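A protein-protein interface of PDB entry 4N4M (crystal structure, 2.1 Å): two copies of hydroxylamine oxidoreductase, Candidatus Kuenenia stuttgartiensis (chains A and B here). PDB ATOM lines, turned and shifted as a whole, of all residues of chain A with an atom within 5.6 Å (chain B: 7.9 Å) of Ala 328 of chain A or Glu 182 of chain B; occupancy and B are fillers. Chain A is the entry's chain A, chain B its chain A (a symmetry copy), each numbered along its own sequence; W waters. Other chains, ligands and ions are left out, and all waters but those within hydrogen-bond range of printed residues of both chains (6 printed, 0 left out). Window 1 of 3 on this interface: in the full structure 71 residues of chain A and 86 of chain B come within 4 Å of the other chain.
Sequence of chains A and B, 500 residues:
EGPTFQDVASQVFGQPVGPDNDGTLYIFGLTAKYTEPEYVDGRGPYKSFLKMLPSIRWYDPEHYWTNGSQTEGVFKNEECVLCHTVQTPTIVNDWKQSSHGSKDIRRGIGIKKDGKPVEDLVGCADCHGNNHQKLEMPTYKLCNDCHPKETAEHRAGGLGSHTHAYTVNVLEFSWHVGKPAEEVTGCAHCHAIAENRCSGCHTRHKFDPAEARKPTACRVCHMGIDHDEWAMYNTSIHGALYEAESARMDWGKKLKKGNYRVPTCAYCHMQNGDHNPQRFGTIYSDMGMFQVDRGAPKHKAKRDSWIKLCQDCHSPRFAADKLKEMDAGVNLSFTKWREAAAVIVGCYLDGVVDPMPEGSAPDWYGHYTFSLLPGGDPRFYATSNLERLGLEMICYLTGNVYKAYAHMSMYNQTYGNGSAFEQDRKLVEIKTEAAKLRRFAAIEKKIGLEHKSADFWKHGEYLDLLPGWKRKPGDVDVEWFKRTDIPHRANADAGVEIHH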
ATOM      1  N   LEU A 323     -20.067   5.808  -3.776  1.00  0.00           N
ATOM      2  CA  LEU A 323     -20.375   7.193  -4.114  1.00  0.00           C
ATOM      3  C   LEU A 323     -19.100   7.950  -4.504  1.00  0.00           C
ATOM      4  O   LEU A 323     -19.152   8.884  -5.304  1.00  0.00           O
ATOM      5  CB  LEU A 323     -21.131   7.867  -2.966  1.00  0.00           C
ATOM      6  CG  LEU A 323     -22.509   7.232  -2.728  1.00  0.00           C
ATOM      7  CD1 LEU A 323     -23.096   7.619  -1.386  1.00  0.00           C
ATOM      8  CD2 LEU A 323     -23.466   7.595  -3.860  1.00  0.00           C
ATOM      9  N   LYS A 324     -17.955   7.526  -3.971  1.00  0.00           N
ATOM     10  CA  LYS A 324     -16.662   8.071  -4.410  1.00  0.00           C
ATOM     11  C   LYS A 324     -16.322   7.623  -5.830  1.00  0.00           C
ATOM     12  O   LYS A 324     -15.711   8.378  -6.585  1.00  0.00           O
ATOM     13  CB  LYS A 324     -15.533   7.676  -3.452  1.00  0.00           C
ATOM     14  CG  LYS A 324     -15.511   8.468  -2.156  1.00  0.00           C
ATOM     15  CD  LYS A 324     -14.504   7.868  -1.179  1.00  0.00           C
ATOM     16  CE  LYS A 324     -14.581   8.524   0.193  1.00  0.00           C
ATOM     17  NZ  LYS A 324     -13.805   7.739   1.197  1.00  0.00           N
ATOM     18  N   GLU A 325     -16.712   6.400  -6.193  1.00  0.00           N
ATOM     19  CA  GLU A 325     -16.568   5.940  -7.576  1.00  0.00           C
ATOM     20  C   GLU A 325     -17.382   6.806  -8.512  1.00  0.00           C
ATOM     21  O   GLU A 325     -16.952   7.091  -9.627  1.00  0.00           O
ATOM     22  CB  GLU A 325     -17.022   4.487  -7.741  1.00  0.00           C
ATOM     23  CG  GLU A 325     -16.128   3.474  -7.072  1.00  0.00           C
ATOM     24  CD  GLU A 325     -16.740   2.081  -7.040  1.00  0.00           C
ATOM     25  OE1 GLU A 325     -17.755   1.832  -7.733  1.00  0.00           O
ATOM     26  OE2 GLU A 325     -16.191   1.230  -6.320  1.00  0.00           O
ATOM     27  N   MET A 326     -18.571   7.197  -8.072  1.00  0.00           N
ATOM     28  CA  MET A 326     -19.396   8.112  -8.846  1.00  0.00           C
ATOM     29  C   MET A 326     -18.646   9.411  -9.107  1.00  0.00           C
ATOM     30  O   MET A 326     -18.497   9.829 -10.257  1.00  0.00           O
ATOM     31  CB  MET A 326     -20.711   8.394  -8.120  1.00  0.00           C
ATOM     32  CG  MET A 326     -21.594   9.412  -8.819  1.00  0.00           C
ATOM     33  SD  MET A 326     -23.102   9.747  -7.903  1.00  0.00           S
ATOM     34  CE  MET A 326     -22.437  10.556  -6.440  1.00  0.00           C
ATOM     35  N   ASP A 327     -18.157  10.031  -8.036  1.00  0.00           N
ATOM     36  CA  ASP A 327     -17.435  11.306  -8.141  1.00  0.00           C
ATOM     37  C   ASP A 327     -16.267  11.205  -9.121  1.00  0.00           C
ATOM     38  O   ASP A 327     -16.101  12.064  -9.991  1.00  0.00           O
ATOM     39  CB  ASP A 327     -16.897  11.752  -6.770  1.00  0.00           C
ATOM     40  CG  ASP A 327     -17.972  11.825  -5.702  1.00  0.00           C
ATOM     41  OD1 ASP A 327     -19.140  12.146  -6.025  1.00  0.00           O
ATOM     42  OD2 ASP A 327     -17.640  11.561  -4.524  1.00  0.00           O
ATOM     43  N   ALA A 328     -15.468  10.148  -8.982  1.00  0.00           N
ATOM     44  CA  ALA A 328     -14.306   9.934  -9.852  1.00  0.00           C
ATOM     45  C   ALA A 328     -14.715   9.695 -11.309  1.00  0.00           C
ATOM     46  O   ALA A 328     -14.135  10.272 -12.232  1.00  0.00           O
ATOM     47  CB  ALA A 328     -13.456   8.758  -9.335  1.00  0.00           C
ATOM     48  N   GLY A 329     -15.728   8.855 -11.507  1.00  0.00           N
ATOM     49  CA  GLY A 329     -16.221   8.548 -12.844  1.00  0.00           C
ATOM     50  C   GLY A 329     -16.777   9.758 -13.562  1.00  0.00           C
ATOM     51  O   GLY A 329     -16.545   9.943 -14.760  1.00  0.00           O
ATOM     52  N   VAL A 330     -17.514  10.582 -12.822  1.00  0.00           N
ATOM     53  CA  VAL A 330     -18.079  11.810 -13.367  1.00  0.00           C
ATOM     54  C   VAL A 330     -16.956  12.759 -13.803  1.00  0.00           C
ATOM     55  O   VAL A 330     -16.937  13.224 -14.938  1.00  0.00           O
ATOM     56  CB  VAL A 330     -19.034  12.490 -12.351  1.00  0.00           C
ATOM     57  CG1 VAL A 330     -19.327  13.931 -12.738  1.00  0.00           C
ATOM     58  CG2 VAL A 330     -20.343  11.694 -12.244  1.00  0.00           C
ATOM     59  N   ASN A 331     -16.003  13.012 -12.912  1.00  0.00           N
ATOM     60  CA  ASN A 331     -14.911  13.929 -13.224  1.00  0.00           C
ATOM     61  C   ASN A 331     -14.124  13.497 -14.455  1.00  0.00           C
ATOM     62  O   ASN A 331     -13.756  14.335 -15.274  1.00  0.00           O
ATOM     63  CB  ASN A 331     -13.998  14.121 -12.009  1.00  0.00           C
ATOM     64  CG  ASN A 331     -14.678  14.892 -10.884  1.00  0.00           C
ATOM     65  OD1 ASN A 331     -15.722  15.516 -11.086  1.00  0.00           O
ATOM     66  ND2 ASN A 331     -14.094  14.848  -9.697  1.00  0.00           N
ATOM     67  N   LEU A 332     -13.898  12.194 -14.618  1.00  0.00           N
ATOM     68  CA  LEU A 332     -13.225  11.705 -15.826  1.00  0.00           C
ATOM     69  C   LEU A 332     -14.076  11.980 -17.065  1.00  0.00           C
ATOM     70  O   LEU A 332     -13.547  12.406 -18.096  1.00  0.00           O
ATOM     71  CB  LEU A 332     -12.887  10.211 -15.714  1.00  0.00           C
ATOM     72  CG  LEU A 332     -12.022   9.560 -16.808  1.00  0.00           C
ATOM     73  CD1 LEU A 332     -12.801   9.395 -18.113  1.00  0.00           C
ATOM     74  CD2 LEU A 332     -10.705  10.314 -17.056  1.00  0.00           C
ATOM     75  N   SER A 333     -15.389  11.758 -16.957  1.00  0.00           N
ATOM     76  CA  SER A 333     -16.297  11.949 -18.095  1.00  0.00           C
ATOM     77  C   SER A 333     -16.244  13.369 -18.667  1.00  0.00           C
ATOM     78  O   SER A 333     -16.405  13.560 -19.874  1.00  0.00           O
ATOM     79  CB  SER A 333     -17.753  11.595 -17.722  1.00  0.00           C
ATOM     80  OG  SER A 333     -18.364  12.595 -16.917  1.00  0.00           O
ATOM     81  N   TYR A 405     -23.501   5.877 -12.684  1.00  0.00           N
ATOM     82  CA  TYR A 405     -22.775   5.727 -11.432  1.00  0.00           C
ATOM     83  C   TYR A 405     -23.694   5.845 -10.208  1.00  0.00           C
ATOM     84  O   TYR A 405     -23.594   5.042  -9.280  1.00  0.00           O
ATOM     85  CB  TYR A 405     -21.627   6.732 -11.342  1.00  0.00           C
ATOM     86  CG  TYR A 405     -20.368   6.276 -12.061  1.00  0.00           C
ATOM     87  CD1 TYR A 405     -20.018   6.801 -13.302  1.00  0.00           C
ATOM     88  CD2 TYR A 405     -19.531   5.314 -11.498  1.00  0.00           C
ATOM     89  CE1 TYR A 405     -18.866   6.377 -13.967  1.00  0.00           C
ATOM     90  CE2 TYR A 405     -18.376   4.889 -12.150  1.00  0.00           C
ATOM     91  CZ  TYR A 405     -18.050   5.423 -13.382  1.00  0.00           C
ATOM     92  OH  TYR A 405     -16.908   5.004 -14.035  1.00  0.00           O
ATOM     93  N   ASP B  20     -11.793  20.333 -10.451  1.00  0.00           N
ATOM     94  CA  ASP B  20     -13.086  19.653 -10.522  1.00  0.00           C
ATOM     95  C   ASP B  20     -13.604  19.177  -9.159  1.00  0.00           C
ATOM     96  O   ASP B  20     -14.812  19.100  -8.954  1.00  0.00           O
ATOM     97  CB  ASP B  20     -13.043  18.492 -11.531  1.00  0.00           C
ATOM     98  CG  ASP B  20     -11.929  17.482 -11.250  1.00  0.00           C
ATOM     99  OD1 ASP B  20     -11.685  16.633 -12.136  1.00  0.00           O
ATOM    100  OD2 ASP B  20     -11.304  17.524 -10.165  1.00  0.00           O
ATOM    101  N   TYR B  34      -9.259  18.874 -14.517  1.00  0.00           N
ATOM    102  CA  TYR B  34      -9.171  17.476 -14.093  1.00  0.00           C
ATOM    103  C   TYR B  34      -8.142  17.282 -12.987  1.00  0.00           C
ATOM    104  O   TYR B  34      -7.013  17.761 -13.094  1.00  0.00           O
ATOM    105  CB  TYR B  34      -8.806  16.579 -15.278  1.00  0.00           C
ATOM    106  CG  TYR B  34      -8.540  15.140 -14.889  1.00  0.00           C
ATOM    107  CD1 TYR B  34      -9.591  14.269 -14.613  1.00  0.00           C
ATOM    108  CD2 TYR B  34      -7.238  14.654 -14.787  1.00  0.00           C
ATOM    109  CE1 TYR B  34      -9.356  12.947 -14.248  1.00  0.00           C
ATOM    110  CE2 TYR B  34      -6.989  13.334 -14.424  1.00  0.00           C
ATOM    111  CZ  TYR B  34      -8.054  12.484 -14.156  1.00  0.00           C
ATOM    112  OH  TYR B  34      -7.822  11.177 -13.799  1.00  0.00           O
ATOM    113  N   THR B  35      -8.545  16.586 -11.925  1.00  0.00           N
ATOM    114  CA  THR B  35      -7.621  16.134 -10.888  1.00  0.00           C
ATOM    115  C   THR B  35      -7.651  14.610 -10.814  1.00  0.00           C
ATOM    116  O   THR B  35      -8.696  13.989 -11.035  1.00  0.00           O
ATOM    117  CB  THR B  35      -8.005  16.678  -9.508  1.00  0.00           C
ATOM    118  OG1 THR B  35      -9.301  16.185  -9.144  1.00  0.00           O
ATOM    119  CG2 THR B  35      -8.007  18.204  -9.513  1.00  0.00           C
ATOM    120  N   GLU B  36      -6.512  14.014 -10.489  1.00  0.00           N
ATOM    121  CA  GLU B  36      -6.448  12.572 -10.305  1.00  0.00           C
ATOM    122  C   GLU B  36      -7.149  12.186  -9.022  1.00  0.00           C
ATOM    123  O   GLU B  36      -6.934  12.819  -7.995  1.00  0.00           O
ATOM    124  CB  GLU B  36      -5.002  12.080 -10.223  1.00  0.00           C
ATOM    125  CG  GLU B  36      -4.387  11.786 -11.560  1.00  0.00           C
ATOM    126  CD  GLU B  36      -3.051  11.073 -11.451  1.00  0.00           C
ATOM    127  OE1 GLU B  36      -2.367  10.988 -12.487  1.00  0.00           O
ATOM    128  OE2 GLU B  36      -2.687  10.605 -10.346  1.00  0.00           O
ATOM    129  N   PRO B  37      -7.983  11.137  -9.067  1.00  0.00           N
ATOM    130  CA  PRO B  37      -8.469  10.570  -7.819  1.00  0.00           C
ATOM    131  C   PRO B  37      -7.352   9.815  -7.108  1.00  0.00           C
ATOM    132  O   PRO B  37      -6.304   9.560  -7.705  1.00  0.00           O
ATOM    133  CB  PRO B  37      -9.564   9.603  -8.277  1.00  0.00           C
ATOM    134  CG  PRO B  37      -9.207   9.246  -9.653  1.00  0.00           C
ATOM    135  CD  PRO B  37      -8.551  10.453 -10.242  1.00  0.00           C
ATOM    136  N   GLU B  38      -7.571   9.470  -5.844  1.00  0.00           N
ATOM    137  CA  GLU B  38      -6.624   8.630  -5.121  1.00  0.00           C
ATOM    138  C   GLU B  38      -6.594   7.269  -5.812  1.00  0.00           C
ATOM    139  O   GLU B  38      -7.642   6.732  -6.161  1.00  0.00           O
ATOM    140  CB  GLU B  38      -7.028   8.462  -3.651  1.00  0.00           C
ATOM    141  CG  GLU B  38      -5.897   7.905  -2.771  1.00  0.00           C
ATOM    142  CD  GLU B  38      -6.404   7.174  -1.528  1.00  0.00           C
ATOM    143  OE1 GLU B  38      -5.844   6.096  -1.206  1.00  0.00           O
ATOM    144  OE2 GLU B  38      -7.358   7.667  -0.880  1.00  0.00           O
ATOM    145  N   TYR B  39      -5.396   6.737  -6.030  1.00  0.00           N
ATOM    146  CA  TYR B  39      -5.226   5.428  -6.654  1.00  0.00           C
ATOM    147  C   TYR B  39      -4.502   4.478  -5.714  1.00  0.00           C
ATOM    148  O   TYR B  39      -3.810   4.903  -4.796  1.00  0.00           O
ATOM    149  CB  TYR B  39      -4.392   5.535  -7.939  1.00  0.00           C
ATOM    150  CG  TYR B  39      -5.047   6.210  -9.130  1.00  0.00           C
ATOM    151  CD1 TYR B  39      -6.367   5.943  -9.491  1.00  0.00           C
ATOM    152  CD2 TYR B  39      -4.317   7.086  -9.932  1.00  0.00           C
ATOM    153  CE1 TYR B  39      -6.944   6.554 -10.603  1.00  0.00           C
ATOM    154  CE2 TYR B  39      -4.883   7.695 -11.045  1.00  0.00           C
ATOM    155  CZ  TYR B  39      -6.194   7.432 -11.377  1.00  0.00           C
ATOM    156  OH  TYR B  39      -6.734   8.048 -12.486  1.00  0.00           O
ATOM    157  N   LYS B  51      -3.455   1.212 -12.438  1.00  0.00           N
ATOM    158  CA  LYS B  51      -4.012   1.704 -11.175  1.00  0.00           C
ATOM    159  C   LYS B  51      -5.424   1.168 -10.982  1.00  0.00           C
ATOM    160  O   LYS B  51      -6.085   0.786 -11.944  1.00  0.00           O
ATOM    161  CB  LYS B  51      -4.039   3.240 -11.154  1.00  0.00           C
ATOM    162  CG  LYS B  51      -2.689   3.919 -11.425  1.00  0.00           C
ATOM    163  CD  LYS B  51      -1.665   3.592 -10.338  1.00  0.00           C
ATOM    164  CE  LYS B  51      -0.290   4.179 -10.645  1.00  0.00           C
ATOM    165  NZ  LYS B  51       0.716   3.788  -9.607  1.00  0.00           N
ATOM    166  N   MET B  52      -5.849   1.126  -9.722  1.00  0.00           N
ATOM    167  CA  MET B  52      -7.225   0.839  -9.333  1.00  0.00           C
ATOM    168  C   MET B  52      -7.661   1.932  -8.369  1.00  0.00           C
ATOM    169  O   MET B  52      -6.824   2.511  -7.678  1.00  0.00           O
ATOM    170  CB  MET B  52      -7.311  -0.510  -8.600  1.00  0.00           C
ATOM    171  CG  MET B  52      -7.073  -1.737  -9.469  1.00  0.00           C
ATOM    172  SD  MET B  52      -8.441  -2.010 -10.603  1.00  0.00           S
ATOM    173  CE  MET B  52      -7.782  -3.297 -11.671  1.00  0.00           C
ATOM    174  N   LEU B  53      -8.964   2.206  -8.302  1.00  0.00           N
ATOM    175  CA  LEU B  53      -9.501   3.011  -7.211  1.00  0.00           C
ATOM    176  C   LEU B  53      -9.457   2.154  -5.943  1.00  0.00           C
ATOM    177  O   LEU B  53      -9.515   0.922  -6.030  1.00  0.00           O
ATOM    178  CB  LEU B  53     -10.936   3.481  -7.500  1.00  0.00           C
ATOM    179  CG  LEU B  53     -11.125   4.517  -8.615  1.00  0.00           C
ATOM    180  CD1 LEU B  53     -12.609   4.856  -8.789  1.00  0.00           C
ATOM    181  CD2 LEU B  53     -10.326   5.785  -8.344  1.00  0.00           C
ATOM    182  N   PRO B  54      -9.355   2.790  -4.760  1.00  0.00           N
ATOM    183  CA  PRO B  54      -9.212   2.022  -3.517  1.00  0.00           C
ATOM    184  C   PRO B  54     -10.374   1.076  -3.209  1.00  0.00           C
ATOM    185  O   PRO B  54     -10.212   0.146  -2.423  1.00  0.00           O
ATOM    186  CB  PRO B  54      -9.113   3.111  -2.442  1.00  0.00           C
ATOM    187  CG  PRO B  54      -8.620   4.304  -3.151  1.00  0.00           C
ATOM    188  CD  PRO B  54      -9.240   4.238  -4.516  1.00  0.00           C
ATOM    189  N   HIS B 176      -8.940  -2.197 -20.682  1.00  0.00           N
ATOM    190  CA  HIS B 176      -8.843  -1.856 -19.270  1.00  0.00           C
ATOM    191  C   HIS B 176      -7.522  -1.171 -18.922  1.00  0.00           C
ATOM    192  O   HIS B 176      -7.512  -0.125 -18.269  1.00  0.00           O
ATOM    193  CB  HIS B 176      -9.009  -3.094 -18.389  1.00  0.00           C
ATOM    194  CG  HIS B 176      -9.288  -2.761 -16.960  1.00  0.00           C
ATOM    195  ND1 HIS B 176     -10.563  -2.552 -16.480  1.00  0.00           N
ATOM    196  CD2 HIS B 176      -8.454  -2.550 -15.917  1.00  0.00           C
ATOM    197  CE1 HIS B 176     -10.500  -2.240 -15.200  1.00  0.00           C
ATOM    198  NE2 HIS B 176      -9.233  -2.237 -14.833  1.00  0.00           N
ATOM    199  N   LYS B 179      -6.772   2.592 -20.208  1.00  0.00           N
ATOM    200  CA  LYS B 179      -7.652   3.681 -19.789  1.00  0.00           C
ATOM    201  C   LYS B 179      -7.419   4.056 -18.333  1.00  0.00           C
ATOM    202  O   LYS B 179      -6.973   3.224 -17.543  1.00  0.00           O
ATOM    203  CB  LYS B 179      -9.121   3.292 -20.004  1.00  0.00           C
ATOM    204  CG  LYS B 179      -9.540   3.253 -21.465  1.00  0.00           C
ATOM    205  CD  LYS B 179     -11.011   2.873 -21.628  1.00  0.00           C
ATOM    206  CE  LYS B 179     -11.535   3.257 -22.998  1.00  0.00           C
ATOM    207  NZ  LYS B 179     -11.735   4.734 -23.140  1.00  0.00           N
ATOM    208  N   PRO B 180      -7.721   5.315 -17.966  1.00  0.00           N
ATOM    209  CA  PRO B 180      -7.650   5.716 -16.559  1.00  0.00           C
ATOM    210  C   PRO B 180      -8.537   4.834 -15.691  1.00  0.00           C
ATOM    211  O   PRO B 180      -9.649   4.483 -16.103  1.00  0.00           O
ATOM    212  CB  PRO B 180      -8.172   7.151 -16.571  1.00  0.00           C
ATOM    213  CG  PRO B 180      -7.943   7.628 -17.955  1.00  0.00           C
ATOM    214  CD  PRO B 180      -8.099   6.440 -18.839  1.00  0.00           C
ATOM    215  N   ALA B 181      -8.037   4.477 -14.510  1.00  0.00           N
ATOM    216  CA  ALA B 181      -8.681   3.484 -13.653  1.00  0.00           C
ATOM    217  C   ALA B 181     -10.154   3.796 -13.396  1.00  0.00           C
ATOM    218  O   ALA B 181     -10.998   2.903 -13.475  1.00  0.00           O
ATOM    219  CB  ALA B 181      -7.933   3.365 -12.324  1.00  0.00           C
ATOM    220  N   GLU B 182     -10.455   5.064 -13.104  1.00  0.00           N
ATOM    221  CA  GLU B 182     -11.810   5.458 -12.707  1.00  0.00           C
ATOM    222  C   GLU B 182     -12.821   5.400 -13.858  1.00  0.00           C
ATOM    223  O   GLU B 182     -14.022   5.428 -13.619  1.00  0.00           O
ATOM    224  CB  GLU B 182     -11.816   6.850 -12.046  1.00  0.00           C
ATOM    225  CG  GLU B 182     -11.619   8.050 -12.995  1.00  0.00           C
ATOM    226  CD  GLU B 182     -10.177   8.545 -13.077  1.00  0.00           C
ATOM    227  OE1 GLU B 182      -9.982   9.776 -13.200  1.00  0.00           O
ATOM    228  OE2 GLU B 182      -9.246   7.714 -13.018  1.00  0.00           O
ATOM    229  N   GLU B 183     -12.337   5.331 -15.097  1.00  0.00           N
ATOM    230  CA  GLU B 183     -13.210   5.173 -16.259  1.00  0.00           C
ATOM    231  C   GLU B 183     -13.778   3.751 -16.354  1.00  0.00           C
ATOM    232  O   GLU B 183     -14.889   3.549 -16.868  1.00  0.00           O
ATOM    233  CB  GLU B 183     -12.459   5.519 -17.549  1.00  0.00           C
ATOM    234  CG  GLU B 183     -13.327   5.509 -18.806  1.00  0.00           C
ATOM    235  CD  GLU B 183     -12.557   5.809 -20.082  1.00  0.00           C
ATOM    236  OE1 GLU B 183     -13.172   5.744 -21.167  1.00  0.00           O
ATOM    237  OE2 GLU B 183     -11.347   6.105 -20.011  1.00  0.00           O
ATOM    238  N   VAL B 184     -13.024   2.780 -15.838  1.00  0.00           N
ATOM    239  CA  VAL B 184     -13.320   1.365 -16.048  1.00  0.00           C
ATOM    240  C   VAL B 184     -13.500   0.567 -14.744  1.00  0.00           C
ATOM    241  O   VAL B 184     -13.391  -0.658 -14.737  1.00  0.00           O
ATOM    242  CB  VAL B 184     -12.237   0.724 -16.952  1.00  0.00           C
ATOM    243  CG1 VAL B 184     -12.258   1.389 -18.333  1.00  0.00           C
ATOM    244  CG2 VAL B 184     -10.851   0.838 -16.323  1.00  0.00           C
ATOM    245  N   THR B 185     -13.804   1.268 -13.652  1.00  0.00           N
ATOM    246  CA  THR B 185     -14.139   0.634 -12.376  1.00  0.00           C
ATOM    247  C   THR B 185     -15.178  -0.480 -12.552  1.00  0.00           C
ATOM    248  O   THR B 185     -15.026  -1.577 -12.009  1.00  0.00           O
ATOM    249  CB  THR B 185     -14.684   1.680 -11.375  1.00  0.00           C
ATOM    250  OG1 THR B 185     -13.686   2.684 -11.141  1.00  0.00           O
ATOM    251  CG2 THR B 185     -15.057   1.023 -10.053  1.00  0.00           C
ATOM    252  N   GLY B 186     -16.222  -0.193 -13.330  1.00  0.00           N
ATOM    253  CA  GLY B 186     -17.303  -1.146 -13.568  1.00  0.00           C
ATOM    254  C   GLY B 186     -16.862  -2.427 -14.260  1.00  0.00           C
ATOM    255  O   GLY B 186     -17.450  -3.489 -14.046  1.00  0.00           O
ATOM    256  N   LEU B 465      -4.187  11.882 -20.948  1.00  0.00           N
ATOM    257  CA  LEU B 465      -4.179  11.034 -19.749  1.00  0.00           C
ATOM    258  C   LEU B 465      -3.860   9.571 -20.050  1.00  0.00           C
ATOM    259  O   LEU B 465      -3.657   8.783 -19.125  1.00  0.00           O
ATOM    260  CB  LEU B 465      -5.537  11.088 -19.049  1.00  0.00           C
ATOM    261  CG  LEU B 465      -6.067  12.453 -18.611  1.00  0.00           C
ATOM    262  CD1 LEU B 465      -7.510  12.315 -18.105  1.00  0.00           C
ATOM    263  CD2 LEU B 465      -5.172  13.075 -17.552  1.00  0.00           C
HETATM  264  O   HOH W   1     -15.060   5.117 -11.089  1.00  0.00           O
HETATM  265  O   HOH W   2     -11.704  11.297 -11.787  1.00  0.00           O
HETATM  266  O   HOH W   3     -16.940   5.282 -16.619  1.00  0.00           O
HETATM  267  O   HOH W   4     -11.413  13.233  -9.948  1.00  0.00           O
HETATM  268  O   HOH W   5     -17.244   2.272 -14.241  1.00  0.00           O
HETATM  269  O   HOH W   6     -12.856  16.711 -14.429  1.00  0.00           O
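O of Glu 182 of chain B is in hydrogen-bond range of OH of Tyr 405 of chain A.
The backbone carbonyl oxygen (O) of Asp 327 of chain A sits close to the side-chain amide nitrogen (ND2) of Asn 331 of chain A, 3.4 Å away. OE1 of Glu 182 of chain B lies within hydrogen-bond range of OH of Tyr 34 of chain B, at 2.6 Å. The side-chain amino group (NZ) of Lys 179 of chain B is in salt-bridge range of the side-chain carboxylate (OE1) of Glu 183 of chain B (2.6 Å). The side-chain carboxylate of Asp 20 of chain B lies within hydrogen-bond range of the side-chain hydroxyl of Thr 35 of chain B, at 2.6 Å. The side-chain hydroxyl (OH) of Tyr 39 of chain B sits at hydrogen-bond distance from the side-chain carboxylate (OE2) of Glu 182 of chain B (2.6 Å).
Glu 325 of chain A touches Thr 185 of chain B (CD to CG2, 3.6 Å). O of Ala 328 of chain A touches CG of Glu 182 of chain B, 3.4 Å away. CA of Gly 329 of chain A touches O of Glu 182 of chain B, 3.9 Å away. Asp 20 of chain B touches Asn 331 of chain A (OD1 to CB, 3.4 Å). Leu 332 of chain A touches Pro 180 of chain B. Leu 332 of chain A touches Glu 182 of chain B (CB to CG, 3.7 Å). Glu 183 of chain B touches Leu 332 of chain A. Leu 332 of chain A touches Leu 465 of chain B (CD2 to CD1, 3.9 Å). Tyr 405 of chain A touches Glu 183 of chain B (OH to O, 3.8 Å).
Of the printed residues of chain B, Ala 328 of chain A touches Glu 182. Glu 182 of chain B touches just these residues of chain A: Ala 328, Gly 329, Leu 332 and Tyr 405. Gly 329 of chain A touches one residue of chain B. Of the printed residues of chain B, Glu 325 of chain A touches Thr 185 (3.6 Å). Of the printed residues of chain A, Glu 183 of chain B touches Leu 332 (3.9 Å) and Tyr 405 (3.8 Å). Printed residues of chain A within 4 Å of Thr 185 of chain B: Glu 325 (3.6 Å). Printed residues of chain A within 4 Å of Pro 180 of chain B: Leu 332. Lys 179 of chain B touches none of the printed residues of chain A. Pro 37 of chain B touches none of the printed residues of chain A. The nearest residue of chain A that does not touch Glu 182 of chain B is Glu 325 of chain A (5.2 Å).
Along chain A the printed residues that touch a printed residue of chain B span positions 325 to 405. Of the 21 printed residues of chain B, 6 touch a printed residue of chain A. Printed residues of chain B that touch a printed residue of chain A: Asp 20, Pro 180, Glu 182, Glu 183, Thr 185 and Leu 465. Among the printed residues, 10 pairs touch across the chains.
No position is printed for both chains. Of the 10 pairs that touch across the chains among the printed residues, none has its exchanged pair printed and touching as well.
Water W6 lies within hydrogen-bond range of the side-chain carboxylate (OD1) of Asp 20 of chain B (2.6 Å) and the backbone carbonyl oxygen (O) of Asn 331 of chain A (2.7 Å). Water W3 lies within hydrogen-bond range of the side-chain hydroxyl of Tyr 405 of chain A (2.6 Å) and the backbone carbonyl oxygen of Glu 183 of chain B (2.7 Å). Water W2 lies within hydrogen-bond range of the backbone carbonyl oxygen (O) of Ala 328 of chain A (2.7 Å) and the side-chain carboxylate (OE1) of Glu 182 of chain B (2.7 Å). Water W1 lies within hydrogen-bond range of O of Glu 182 of chain B (2.8 Å), OG1 of Thr 185 of chain B (2.8 Å), O of Glu 325 of chain A (3.1 Å) and OH of Tyr 405 of chain A (3.5 Å). Water W5 bridges the side-chain hydroxyl (OH) of Tyr 405 of chain A (2.8 Å) and the backbone NH (N) of Gly 186 of chain B (2.8 Å). Water W4 bridges O of Thr 35 of chain B and ND2 of Asn 331 of chain A.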
